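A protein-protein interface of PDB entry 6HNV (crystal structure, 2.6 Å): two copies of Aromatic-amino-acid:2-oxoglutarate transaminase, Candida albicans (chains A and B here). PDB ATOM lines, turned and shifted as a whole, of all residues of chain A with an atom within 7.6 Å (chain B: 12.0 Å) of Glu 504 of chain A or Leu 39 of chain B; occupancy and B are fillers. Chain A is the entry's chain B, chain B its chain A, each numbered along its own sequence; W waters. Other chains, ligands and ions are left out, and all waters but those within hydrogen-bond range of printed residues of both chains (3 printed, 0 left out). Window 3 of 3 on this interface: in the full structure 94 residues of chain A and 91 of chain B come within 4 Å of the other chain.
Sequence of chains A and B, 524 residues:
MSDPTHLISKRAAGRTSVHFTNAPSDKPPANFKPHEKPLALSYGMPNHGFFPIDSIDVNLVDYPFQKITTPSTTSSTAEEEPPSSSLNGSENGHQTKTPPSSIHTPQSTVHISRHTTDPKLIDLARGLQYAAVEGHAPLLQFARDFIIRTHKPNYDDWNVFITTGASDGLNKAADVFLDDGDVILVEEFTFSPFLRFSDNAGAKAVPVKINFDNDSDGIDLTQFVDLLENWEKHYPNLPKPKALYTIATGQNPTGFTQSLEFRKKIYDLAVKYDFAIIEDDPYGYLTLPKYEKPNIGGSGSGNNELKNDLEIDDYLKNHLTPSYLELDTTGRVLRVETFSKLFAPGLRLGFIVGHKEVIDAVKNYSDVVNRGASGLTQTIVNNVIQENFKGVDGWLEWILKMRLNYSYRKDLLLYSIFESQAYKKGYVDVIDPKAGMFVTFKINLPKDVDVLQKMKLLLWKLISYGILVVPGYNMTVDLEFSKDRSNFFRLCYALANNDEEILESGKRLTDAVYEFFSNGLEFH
Water W3 bridges OG of Ser 505 of chain A and O of Ala 40 of chain B.
Water W1 lies within hydrogen-bond range of O of Lys 37 of chain B (3.0 Å) and NH2 of Arg 508 of chain A (3.0 Å).
Printed residues of chain A that touch a printed residue of chain B: Leu 413, Tyr 465, Gly 466, Ile 467, Leu 468, Val 469, Leu 495, Ala 496, Asn 497, Glu 501, Glu 504, Ser 505 and Arg 508.
Hydrophobic or aromatic side chains of chain A within 4 Å of the printed part of chain B: Leu 413, Ile 467, Leu 468 and Leu 495.
Among the printed residues, no Asp or Glu carboxylate lies within 4 Å of a Lys or Arg side-chain nitrogen of the other chain.
The backbone carbonyl oxygen (O) of Lys 37 of chain B sits at hydrogen-bond distance from the guanidinium group (NH1) of Arg 508 of chain A, 3.4 Å away.
The side-chain amide nitrogen (ND2) of Asn 47 of chain B sits at hydrogen-bond distance from the backbone carbonyl oxygen (O) of Leu 495 of chain A (2.9 Å).
The backbone carbonyl oxygen (O) of Leu 39 of chain B is in hydrogen-bond range of the backbone NH (N) of Leu 468 of chain A, 3.1 Å away.
N of Leu 39 of chain B sits at hydrogen-bond distance from O of Gly 466 of chain A, 2.9 Å away.
The side-chain amide nitrogen of Asn 47 of chain B is in hydrogen-bond range of the side-chain amide oxygen of Asn 497 of chain A, 2.7 Å away.
N of Leu 41 of chain B sits at hydrogen-bond distance from O of Leu 468 of chain A, at 2.9 Å.
The side-chain carboxylate of Glu 501 of chain A lies within hydrogen-bond range of the backbone NH of Asn 497 of chain A, 2.9 Å away.
No position is printed for both chains.
Of the 25 pairs that touch across the chains among the printed residues, none has its exchanged pair printed and touching as well.
Ile 467 of chain A touches two residues of chain B.
No residue of chain B comes within 4 Å of Gly 506 of chain A.
No residue of chain B comes within 4 Å of Lys 507 of chain A.
Printed residues of chain A within 4 Å of Met 45 of chain B: Leu 495.
Printed residues of chain A within 4 Å of Asn 47 of chain B: Leu 495 (2.9 Å), Ala 496 (3.5 Å) and Asn 497 (2.7 Å).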
ATOM      1  N   LEU A 413     -10.148  22.576   6.820  1.00  0.00           N
ATOM      2  CA  LEU A 413      -8.781  22.316   6.301  1.00  0.00           C
ATOM      3  C   LEU A 413      -8.828  21.094   5.386  1.00  0.00           C
ATOM      4  O   LEU A 413      -8.199  21.112   4.320  1.00  0.00           O
ATOM      5  CB  LEU A 413      -7.825  22.093   7.472  1.00  0.00           C
ATOM      6  CG  LEU A 413      -6.366  21.940   7.073  1.00  0.00           C
ATOM      7  CD1 LEU A 413      -5.920  23.167   6.299  1.00  0.00           C
ATOM      8  CD2 LEU A 413      -5.493  21.704   8.297  1.00  0.00           C
ATOM      9  N   SER A 416     -10.810  21.887   2.206  1.00  0.00           N
ATOM     10  CA  SER A 416      -9.725  22.684   1.595  1.00  0.00           C
ATOM     11  C   SER A 416      -8.858  21.788   0.714  1.00  0.00           C
ATOM     12  O   SER A 416      -8.594  22.159  -0.430  1.00  0.00           O
ATOM     13  CB  SER A 416      -8.918  23.326   2.687  1.00  0.00           C
ATOM     14  OG  SER A 416      -8.112  24.352   2.161  1.00  0.00           O
ATOM     15  N   LEU A 462       6.743  25.144  -0.458  1.00  0.00           N
ATOM     16  CA  LEU A 462       5.657  25.579   0.459  1.00  0.00           C
ATOM     17  C   LEU A 462       5.953  27.027   0.877  1.00  0.00           C
ATOM     18  O   LEU A 462       5.080  27.876   0.664  1.00  0.00           O
ATOM     19  CB  LEU A 462       5.520  24.640   1.669  1.00  0.00           C
ATOM     20  CG  LEU A 462       4.928  23.252   1.398  1.00  0.00           C
ATOM     21  CD1 LEU A 462       4.593  22.534   2.700  1.00  0.00           C
ATOM     22  CD2 LEU A 462       3.692  23.320   0.532  1.00  0.00           C
ATOM     23  N   TYR A 465       5.282  29.715  -1.753  1.00  0.00           N
ATOM     24  CA  TYR A 465       3.813  29.885  -1.939  1.00  0.00           C
ATOM     25  C   TYR A 465       3.156  30.533  -0.702  1.00  0.00           C
ATOM     26  O   TYR A 465       1.979  30.900  -0.815  1.00  0.00           O
ATOM     27  CB  TYR A 465       3.153  28.548  -2.293  1.00  0.00           C
ATOM     28  CG  TYR A 465       3.108  28.237  -3.767  1.00  0.00           C
ATOM     29  CD1 TYR A 465       4.262  27.951  -4.479  1.00  0.00           C
ATOM     30  CD2 TYR A 465       1.907  28.237  -4.449  1.00  0.00           C
ATOM     31  CE1 TYR A 465       4.226  27.669  -5.829  1.00  0.00           C
ATOM     32  CE2 TYR A 465       1.854  27.952  -5.801  1.00  0.00           C
ATOM     33  CZ  TYR A 465       3.018  27.673  -6.491  1.00  0.00           C
ATOM     34  OH  TYR A 465       2.951  27.391  -7.822  1.00  0.00           O
ATOM     35  N   GLY A 466       3.865  30.667   0.428  1.00  0.00           N
ATOM     36  CA  GLY A 466       3.404  31.387   1.640  1.00  0.00           C
ATOM     37  C   GLY A 466       2.585  30.542   2.620  1.00  0.00           C
ATOM     38  O   GLY A 466       1.674  31.113   3.260  1.00  0.00           O
ATOM     39  N   ILE A 467       2.910  29.249   2.787  1.00  0.00           N
ATOM     40  CA  ILE A 467       2.312  28.350   3.829  1.00  0.00           C
ATOM     41  C   ILE A 467       3.445  27.665   4.610  1.00  0.00           C
ATOM     42  O   ILE A 467       4.212  26.857   4.031  1.00  0.00           O
ATOM     43  CB  ILE A 467       1.284  27.358   3.225  1.00  0.00           C
ATOM     44  CG1 ILE A 467       0.506  26.601   4.303  1.00  0.00           C
ATOM     45  CG2 ILE A 467       1.923  26.399   2.233  1.00  0.00           C
ATOM     46  CD1 ILE A 467      -0.372  27.476   5.151  1.00  0.00           C
ATOM     47  N   LEU A 468       3.564  28.023   5.886  1.00  0.00           N
ATOM     48  CA  LEU A 468       4.473  27.373   6.849  1.00  0.00           C
ATOM     49  C   LEU A 468       3.776  26.114   7.357  1.00  0.00           C
ATOM     50  O   LEU A 468       2.580  26.212   7.679  1.00  0.00           O
ATOM     51  CB  LEU A 468       4.768  28.367   7.972  1.00  0.00           C
ATOM     52  CG  LEU A 468       5.404  29.682   7.512  1.00  0.00           C
ATOM     53  CD1 LEU A 468       5.676  30.606   8.698  1.00  0.00           C
ATOM     54  CD2 LEU A 468       6.686  29.419   6.729  1.00  0.00           C
ATOM     55  N   VAL A 469       4.492  24.982   7.350  1.00  0.00           N
ATOM     56  CA  VAL A 469       4.091  23.676   7.966  1.00  0.00           C
ATOM     57  C   VAL A 469       5.312  23.127   8.712  1.00  0.00           C
ATOM     58  O   VAL A 469       6.370  23.701   8.525  1.00  0.00           O
ATOM     59  CB  VAL A 469       3.582  22.692   6.893  1.00  0.00           C
ATOM     60  CG1 VAL A 469       2.345  23.212   6.171  1.00  0.00           C
ATOM     61  CG2 VAL A 469       4.673  22.337   5.899  1.00  0.00           C
ATOM     62  N   LEU A 495      -4.019  27.896  15.072  1.00  0.00           N
ATOM     63  CA  LEU A 495      -3.403  29.246  15.182  1.00  0.00           C
ATOM     64  C   LEU A 495      -4.164  30.285  14.335  1.00  0.00           C
ATOM     65  O   LEU A 495      -4.228  31.465  14.762  1.00  0.00           O
ATOM     66  CB  LEU A 495      -1.926  29.156  14.772  1.00  0.00           C
ATOM     67  CG  LEU A 495      -1.124  30.461  14.855  1.00  0.00           C
ATOM     68  CD1 LEU A 495      -1.327  31.204  16.182  1.00  0.00           C
ATOM     69  CD2 LEU A 495       0.351  30.181  14.625  1.00  0.00           C
ATOM     70  N   ALA A 496      -4.716  29.884  13.184  1.00  0.00           N
ATOM     71  CA  ALA A 496      -5.494  30.745  12.258  1.00  0.00           C
ATOM     72  C   ALA A 496      -6.557  31.564  13.004  1.00  0.00           C
ATOM     73  O   ALA A 496      -7.090  31.088  14.032  1.00  0.00           O
ATOM     74  CB  ALA A 496      -6.139  29.890  11.207  1.00  0.00           C
ATOM     75  N   ASN A 497      -6.859  32.747  12.466  1.00  0.00           N
ATOM     76  CA  ASN A 497      -7.778  33.763  13.039  1.00  0.00           C
ATOM     77  C   ASN A 497      -9.218  33.443  12.651  1.00  0.00           C
ATOM     78  O   ASN A 497     -10.124  33.782  13.425  1.00  0.00           O
ATOM     79  CB  ASN A 497      -7.439  35.171  12.548  1.00  0.00           C
ATOM     80  CG  ASN A 497      -6.176  35.712  13.176  1.00  0.00           C
ATOM     81  OD1 ASN A 497      -6.116  35.862  14.387  1.00  0.00           O
ATOM     82  ND2 ASN A 497      -5.165  35.985  12.370  1.00  0.00           N
ATOM     83  N   ASN A 498      -9.426  32.813  11.500  1.00  0.00           N
ATOM     84  CA  ASN A 498     -10.788  32.646  10.935  1.00  0.00           C
ATOM     85  C   ASN A 498     -10.790  31.579   9.835  1.00  0.00           C
ATOM     86  O   ASN A 498      -9.718  31.051   9.496  1.00  0.00           O
ATOM     87  CB  ASN A 498     -11.292  33.986  10.394  1.00  0.00           C
ATOM     88  CG  ASN A 498     -10.313  34.596   9.414  1.00  0.00           C
ATOM     89  OD1 ASN A 498      -9.895  33.937   8.473  1.00  0.00           O
ATOM     90  ND2 ASN A 498      -9.892  35.827   9.658  1.00  0.00           N
ATOM     91  N   ASP A 499     -11.966  31.335   9.267  1.00  0.00           N
ATOM     92  CA  ASP A 499     -12.264  30.222   8.333  1.00  0.00           C
ATOM     93  C   ASP A 499     -11.578  30.463   6.974  1.00  0.00           C
ATOM     94  O   ASP A 499     -11.196  29.468   6.337  1.00  0.00           O
ATOM     95  CB  ASP A 499     -13.788  30.059   8.225  1.00  0.00           C
ATOM     96  CG  ASP A 499     -14.472  29.789   9.558  1.00  0.00           C
ATOM     97  OD1 ASP A 499     -13.865  29.092  10.408  1.00  0.00           O
ATOM     98  OD2 ASP A 499     -15.598  30.295   9.742  1.00  0.00           O
ATOM     99  N   GLU A 500     -11.443  31.722   6.538  1.00  0.00           N
ATOM    100  CA  GLU A 500     -10.950  32.097   5.181  1.00  0.00           C
ATOM    101  C   GLU A 500      -9.448  31.798   5.114  1.00  0.00           C
ATOM    102  O   GLU A 500      -8.968  31.337   4.060  1.00  0.00           O
ATOM    103  CB  GLU A 500     -11.262  33.570   4.881  1.00  0.00           C
ATOM    104  CG  GLU A 500     -12.740  33.862   4.638  1.00  0.00           C
ATOM    105  CD  GLU A 500     -13.708  33.459   5.749  1.00  0.00           C
ATOM    106  OE1 GLU A 500     -13.706  34.114   6.834  1.00  0.00           O
ATOM    107  OE2 GLU A 500     -14.470  32.480   5.533  1.00  0.00           O
ATOM    108  N   GLU A 501      -8.742  32.066   6.213  1.00  0.00           N
ATOM    109  CA  GLU A 501      -7.318  31.698   6.427  1.00  0.00           C
ATOM    110  C   GLU A 501      -7.162  30.184   6.279  1.00  0.00           C
ATOM    111  O   GLU A 501      -6.220  29.802   5.608  1.00  0.00           O
ATOM    112  CB  GLU A 501      -6.807  32.189   7.786  1.00  0.00           C
ATOM    113  CG  GLU A 501      -6.043  33.502   7.700  1.00  0.00           C
ATOM    114  CD  GLU A 501      -5.877  34.267   9.002  1.00  0.00           C
ATOM    115  OE1 GLU A 501      -5.654  33.620  10.026  1.00  0.00           O
ATOM    116  OE2 GLU A 501      -5.970  35.517   8.977  1.00  0.00           O
ATOM    117  N   ILE A 502      -8.054  29.367   6.848  1.00  0.00           N
ATOM    118  CA  ILE A 502      -7.954  27.871   6.784  1.00  0.00           C
ATOM    119  C   ILE A 502      -8.031  27.454   5.317  1.00  0.00           C
ATOM    120  O   ILE A 502      -7.177  26.659   4.882  1.00  0.00           O
ATOM    121  CB  ILE A 502      -9.057  27.141   7.573  1.00  0.00           C
ATOM    122  CG1 ILE A 502      -9.205  27.652   9.007  1.00  0.00           C
ATOM    123  CG2 ILE A 502      -8.832  25.632   7.523  1.00  0.00           C
ATOM    124  CD1 ILE A 502      -7.952  27.524   9.830  1.00  0.00           C
ATOM    125  N   LEU A 503      -9.062  27.959   4.624  1.00  0.00           N
ATOM    126  CA  LEU A 503      -9.302  27.826   3.163  1.00  0.00           C
ATOM    127  C   LEU A 503      -8.055  28.315   2.424  1.00  0.00           C
ATOM    128  O   LEU A 503      -7.565  27.573   1.583  1.00  0.00           O
ATOM    129  CB  LEU A 503     -10.558  28.619   2.765  1.00  0.00           C
ATOM    130  CG  LEU A 503     -11.891  27.970   3.168  1.00  0.00           C
ATOM    131  CD1 LEU A 503     -13.022  28.987   3.274  1.00  0.00           C
ATOM    132  CD2 LEU A 503     -12.282  26.862   2.203  1.00  0.00           C
ATOM    133  N   GLU A 504      -7.534  29.501   2.730  1.00  0.00           N
ATOM    134  CA  GLU A 504      -6.414  30.051   1.922  1.00  0.00           C
ATOM    135  C   GLU A 504      -5.163  29.224   2.248  1.00  0.00           C
ATOM    136  O   GLU A 504      -4.482  28.781   1.285  1.00  0.00           O
ATOM    137  CB  GLU A 504      -6.263  31.567   2.074  1.00  0.00           C
ATOM    138  CG  GLU A 504      -5.198  32.150   1.161  1.00  0.00           C
ATOM    139  CD  GLU A 504      -5.323  31.858  -0.330  1.00  0.00           C
ATOM    140  OE1 GLU A 504      -6.422  31.445  -0.796  1.00  0.00           O
ATOM    141  OE2 GLU A 504      -4.318  32.067  -1.044  1.00  0.00           O
ATOM    142  N   SER A 505      -4.934  28.924   3.530  1.00  0.00           N
ATOM    143  CA  SER A 505      -3.856  28.023   4.019  1.00  0.00           C
ATOM    144  C   SER A 505      -3.787  26.731   3.190  1.00  0.00           C
ATOM    145  O   SER A 505      -2.728  26.466   2.606  1.00  0.00           O
ATOM    146  CB  SER A 505      -4.018  27.761   5.483  1.00  0.00           C
ATOM    147  OG  SER A 505      -3.779  28.971   6.217  1.00  0.00           O
ATOM    148  N   GLY A 506      -4.872  25.967   3.088  1.00  0.00           N
ATOM    149  CA  GLY A 506      -4.877  24.680   2.364  1.00  0.00           C
ATOM    150  C   GLY A 506      -4.955  24.840   0.849  1.00  0.00           C
ATOM    151  O   GLY A 506      -4.665  23.848   0.132  1.00  0.00           O
ATOM    152  N   LYS A 507      -5.360  26.014   0.341  1.00  0.00           N
ATOM    153  CA  LYS A 507      -5.296  26.293  -1.119  1.00  0.00           C
ATOM    154  C   LYS A 507      -3.818  26.262  -1.508  1.00  0.00           C
ATOM    155  O   LYS A 507      -3.449  25.416  -2.320  1.00  0.00           O
ATOM    156  CB  LYS A 507      -5.947  27.630  -1.491  1.00  0.00           C
ATOM    157  CG  LYS A 507      -5.712  28.063  -2.934  1.00  0.00           C
ATOM    158  CD  LYS A 507      -6.711  29.076  -3.462  1.00  0.00           C
ATOM    159  CE  LYS A 507      -6.088  30.051  -4.442  1.00  0.00           C
ATOM    160  NZ  LYS A 507      -5.550  29.366  -5.640  1.00  0.00           N
ATOM    161  N   ARG A 508      -3.026  27.112  -0.851  1.00  0.00           N
ATOM    162  CA  ARG A 508      -1.585  27.334  -1.107  1.00  0.00           C
ATOM    163  C   ARG A 508      -0.836  26.016  -0.912  1.00  0.00           C
ATOM    164  O   ARG A 508      -0.014  25.677  -1.800  1.00  0.00           O
ATOM    165  CB  ARG A 508      -1.014  28.401  -0.164  1.00  0.00           C
ATOM    166  CG  ARG A 508      -1.641  29.789  -0.274  1.00  0.00           C
ATOM    167  CD  ARG A 508      -1.173  30.789   0.789  1.00  0.00           C
ATOM    168  NE  ARG A 508      -1.859  32.077   0.670  1.00  0.00           N
ATOM    169  CZ  ARG A 508      -1.492  33.220   1.247  1.00  0.00           C
ATOM    170  NH1 ARG A 508      -0.415  33.276   2.017  1.00  0.00           N
ATOM    171  NH2 ARG A 508      -2.218  34.308   1.044  1.00  0.00           N
ATOM    172  N   LEU A 509      -1.109  25.307   0.199  1.00  0.00           N
ATOM    173  CA  LEU A 509      -0.421  24.033   0.554  1.00  0.00           C
ATOM    174  C   LEU A 509      -0.544  23.082  -0.636  1.00  0.00           C
ATOM    175  O   LEU A 509       0.495  22.605  -1.115  1.00  0.00           O
ATOM    176  CB  LEU A 509      -1.038  23.442   1.825  1.00  0.00           C
ATOM    177  CG  LEU A 509      -0.597  22.029   2.215  1.00  0.00           C
ATOM    178  CD1 LEU A 509       0.910  21.921   2.260  1.00  0.00           C
ATOM    179  CD2 LEU A 509      -1.177  21.651   3.565  1.00  0.00           C
ATOM    180  N   THR A 510      -1.762  22.891  -1.138  1.00  0.00           N
ATOM    181  CA  THR A 510      -2.070  21.982  -2.282  1.00  0.00           C
ATOM    182  C   THR A 510      -1.683  22.596  -3.638  1.00  0.00           C
ATOM    183  O   THR A 510      -1.349  21.791  -4.542  1.00  0.00           O
ATOM    184  CB  THR A 510      -3.535  21.566  -2.259  1.00  0.00           C
ATOM    185  OG1 THR A 510      -4.267  22.792  -2.213  1.00  0.00           O
ATOM    186  CG2 THR A 510      -3.847  20.672  -1.082  1.00  0.00           C
ATOM    187  N   ASP A 511      -1.719  23.924  -3.803  1.00  0.00           N
ATOM    188  CA  ASP A 511      -1.224  24.585  -5.045  1.00  0.00           C
ATOM    189  C   ASP A 511       0.281  24.288  -5.196  1.00  0.00           C
ATOM    190  O   ASP A 511       0.705  23.847  -6.271  1.00  0.00           O
ATOM    191  CB  ASP A 511      -1.468  26.100  -5.041  1.00  0.00           C
ATOM    192  CG  ASP A 511      -2.884  26.586  -5.338  1.00  0.00           C
ATOM    193  OD1 ASP A 511      -3.761  25.765  -5.729  1.00  0.00           O
ATOM    194  OD2 ASP A 511      -3.104  27.796  -5.156  1.00  0.00           O
ATOM    195  N   PRO B  34      11.049  33.981  -0.643  1.00  0.00           N
ATOM    196  CA  PRO B  34       9.957  33.655   0.272  1.00  0.00           C
ATOM    197  C   PRO B  34       8.717  34.487  -0.098  1.00  0.00           C
ATOM    198  O   PRO B  34       8.898  35.531  -0.691  1.00  0.00           O
ATOM    199  CB  PRO B  34      10.507  34.011   1.668  1.00  0.00           C
ATOM    200  CG  PRO B  34      11.704  34.902   1.407  1.00  0.00           C
ATOM    201  CD  PRO B  34      12.236  34.504   0.045  1.00  0.00           C
ATOM    202  N   HIS B  35       7.507  34.014   0.216  1.00  0.00           N
ATOM    203  CA  HIS B  35       6.241  34.778   0.043  1.00  0.00           C
ATOM    204  C   HIS B  35       6.219  35.873   1.102  1.00  0.00           C
ATOM    205  O   HIS B  35       6.806  35.638   2.157  1.00  0.00           O
ATOM    206  CB  HIS B  35       5.023  33.856   0.143  1.00  0.00           C
ATOM    207  CG  HIS B  35       3.700  34.484  -0.158  1.00  0.00           C
ATOM    208  ND1 HIS B  35       3.047  35.321   0.742  1.00  0.00           N
ATOM    209  CD2 HIS B  35       2.856  34.311  -1.198  1.00  0.00           C
ATOM    210  CE1 HIS B  35       1.880  35.670   0.245  1.00  0.00           C
ATOM    211  NE2 HIS B  35       1.738  35.059  -0.940  1.00  0.00           N
ATOM    212  N   GLU B  36       5.541  36.989   0.814  1.00  0.00           N
ATOM    213  CA  GLU B  36       5.679  38.290   1.527  1.00  0.00           C
ATOM    214  C   GLU B  36       4.845  38.272   2.818  1.00  0.00           C
ATOM    215  O   GLU B  36       5.413  38.576   3.881  1.00  0.00           O
ATOM    216  CB  GLU B  36       5.267  39.425   0.583  1.00  0.00           C
ATOM    217  CG  GLU B  36       6.204  40.622   0.604  1.00  0.00           C
ATOM    218  CD  GLU B  36       5.933  41.620  -0.512  1.00  0.00           C
ATOM    219  OE1 GLU B  36       5.969  41.215  -1.703  1.00  0.00           O
ATOM    220  OE2 GLU B  36       5.666  42.796  -0.191  1.00  0.00           O
ATOM    221  N   LYS B  37       3.549  37.955   2.717  1.00  0.00           N
ATOM    222  CA  LYS B  37       2.601  37.838   3.860  1.00  0.00           C
ATOM    223  C   LYS B  37       2.083  36.402   3.903  1.00  0.00           C
ATOM    224  O   LYS B  37       1.074  36.079   3.275  1.00  0.00           O
ATOM    225  CB  LYS B  37       1.467  38.859   3.726  1.00  0.00           C
ATOM    226  CG  LYS B  37       0.588  39.011   4.962  1.00  0.00           C
ATOM    227  CD  LYS B  37       1.228  39.824   6.079  1.00  0.00           C
ATOM    228  CE  LYS B  37       0.950  39.301   7.478  1.00  0.00           C
ATOM    229  NZ  LYS B  37      -0.496  39.111   7.743  1.00  0.00           N
ATOM    230  N   PRO B  38       2.782  35.498   4.632  1.00  0.00           N
ATOM    231  CA  PRO B  38       2.451  34.073   4.668  1.00  0.00           C
ATOM    232  C   PRO B  38       1.564  33.624   5.840  1.00  0.00           C
ATOM    233  O   PRO B  38       1.425  34.362   6.793  1.00  0.00           O
ATOM    234  CB  PRO B  38       3.843  33.476   4.853  1.00  0.00           C
ATOM    235  CG  PRO B  38       4.499  34.429   5.825  1.00  0.00           C
ATOM    236  CD  PRO B  38       3.968  35.799   5.448  1.00  0.00           C
ATOM    237  N   LEU B  39       0.982  32.424   5.730  1.00  0.00           N
ATOM    238  CA  LEU B  39       0.013  31.860   6.712  1.00  0.00           C
ATOM    239  C   LEU B  39       0.677  30.690   7.442  1.00  0.00           C
ATOM    240  O   LEU B  39       1.726  30.216   6.967  1.00  0.00           O
ATOM    241  CB  LEU B  39      -1.262  31.428   5.976  1.00  0.00           C
ATOM    242  CG  LEU B  39      -2.051  32.553   5.295  1.00  0.00           C
ATOM    243  CD1 LEU B  39      -3.277  31.996   4.596  1.00  0.00           C
ATOM    244  CD2 LEU B  39      -2.470  33.619   6.292  1.00  0.00           C
ATOM    245  N   ALA B  40       0.130  30.279   8.583  1.00  0.00           N
ATOM    246  CA  ALA B  40       0.751  29.255   9.452  1.00  0.00           C
ATOM    247  C   ALA B  40      -0.211  28.084   9.664  1.00  0.00           C
ATOM    248  O   ALA B  40      -1.348  28.298  10.146  1.00  0.00           O
ATOM    249  CB  ALA B  40       1.164  29.876  10.761  1.00  0.00           C
ATOM    250  N   LEU B  41       0.240  26.885   9.306  1.00  0.00           N
ATOM    251  CA  LEU B  41      -0.272  25.594   9.842  1.00  0.00           C
ATOM    252  C   LEU B  41       0.901  24.910  10.547  1.00  0.00           C
ATOM    253  O   LEU B  41       1.022  23.670  10.457  1.00  0.00           O
ATOM    254  CB  LEU B  41      -0.810  24.731   8.690  1.00  0.00           C
ATOM    255  CG  LEU B  41      -1.902  25.358   7.833  1.00  0.00           C
ATOM    256  CD1 LEU B  41      -2.448  24.333   6.861  1.00  0.00           C
ATOM    257  CD2 LEU B  41      -3.015  25.908   8.701  1.00  0.00           C
ATOM    258  N   SER B  42       1.765  25.716  11.170  1.00  0.00           N
ATOM    259  CA  SER B  42       3.061  25.294  11.763  1.00  0.00           C
ATOM    260  C   SER B  42       2.866  25.024  13.259  1.00  0.00           C
ATOM    261  O   SER B  42       2.805  23.845  13.633  1.00  0.00           O
ATOM    262  CB  SER B  42       4.172  26.294  11.492  1.00  0.00           C
ATOM    263  OG  SER B  42       3.774  27.610  11.825  1.00  0.00           O
ATOM    264  N   TYR B  43       2.722  26.064  14.075  1.00  0.00           N
ATOM    265  CA  TYR B  43       2.856  25.950  15.550  1.00  0.00           C
ATOM    266  C   TYR B  43       1.508  25.587  16.189  1.00  0.00           C
ATOM    267  O   TYR B  43       0.458  26.074  15.722  1.00  0.00           O
ATOM    268  CB  TYR B  43       3.497  27.224  16.098  1.00  0.00           C
ATOM    269  CG  TYR B  43       4.891  27.451  15.574  1.00  0.00           C
ATOM    270  CD1 TYR B  43       5.852  26.450  15.653  1.00  0.00           C
ATOM    271  CD2 TYR B  43       5.249  28.652  14.977  1.00  0.00           C
ATOM    272  CE1 TYR B  43       7.137  26.639  15.167  1.00  0.00           C
ATOM    273  CE2 TYR B  43       6.532  28.859  14.491  1.00  0.00           C
ATOM    274  CZ  TYR B  43       7.482  27.850  14.589  1.00  0.00           C
ATOM    275  OH  TYR B  43       8.754  28.030  14.118  1.00  0.00           O
ATOM    276  N   GLY B  44       1.567  24.713  17.205  1.00  0.00           N
ATOM    277  CA  GLY B  44       0.460  24.267  18.078  1.00  0.00           C
ATOM    278  C   GLY B  44       0.129  25.296  19.144  1.00  0.00           C
ATOM    279  O   GLY B  44       0.156  24.947  20.343  1.00  0.00           O
ATOM    280  N   MET B  45      -0.188  26.510  18.688  1.00  0.00           N
ATOM    281  CA  MET B  45      -0.551  27.713  19.480  1.00  0.00           C
ATOM    282  C   MET B  45      -2.036  28.018  19.244  1.00  0.00           C
ATOM    283  O   MET B  45      -2.407  28.423  18.147  1.00  0.00           O
ATOM    284  CB  MET B  45       0.283  28.927  19.029  1.00  0.00           C
ATOM    285  CG  MET B  45       1.794  28.822  19.273  1.00  0.00           C
ATOM    286  SD  MET B  45       2.780  29.929  18.210  1.00  0.00           S
ATOM    287  CE  MET B  45       3.601  30.992  19.404  1.00  0.00           C
ATOM    288  N   ASN B  47      -5.105  30.281  18.768  1.00  0.00           N
ATOM    289  CA  ASN B  47      -5.374  31.726  18.517  1.00  0.00           C
ATOM    290  C   ASN B  47      -5.891  32.339  19.825  1.00  0.00           C
ATOM    291  O   ASN B  47      -6.690  31.663  20.492  1.00  0.00           O
ATOM    292  CB  ASN B  47      -6.371  31.923  17.370  1.00  0.00           C
ATOM    293  CG  ASN B  47      -6.459  33.354  16.886  1.00  0.00           C
ATOM    294  OD1 ASN B  47      -7.363  34.087  17.299  1.00  0.00           O
ATOM    295  ND2 ASN B  47      -5.534  33.758  16.020  1.00  0.00           N
HETATM  296  O   HOH W   1      -1.243  37.122   1.625  1.00  0.00           O
HETATM  297  O   HOH W   2      -3.749  27.323  11.640  1.00  0.00           O
HETATM  298  O   HOH W   3      -3.600  29.284   8.735  1.00  0.00           O
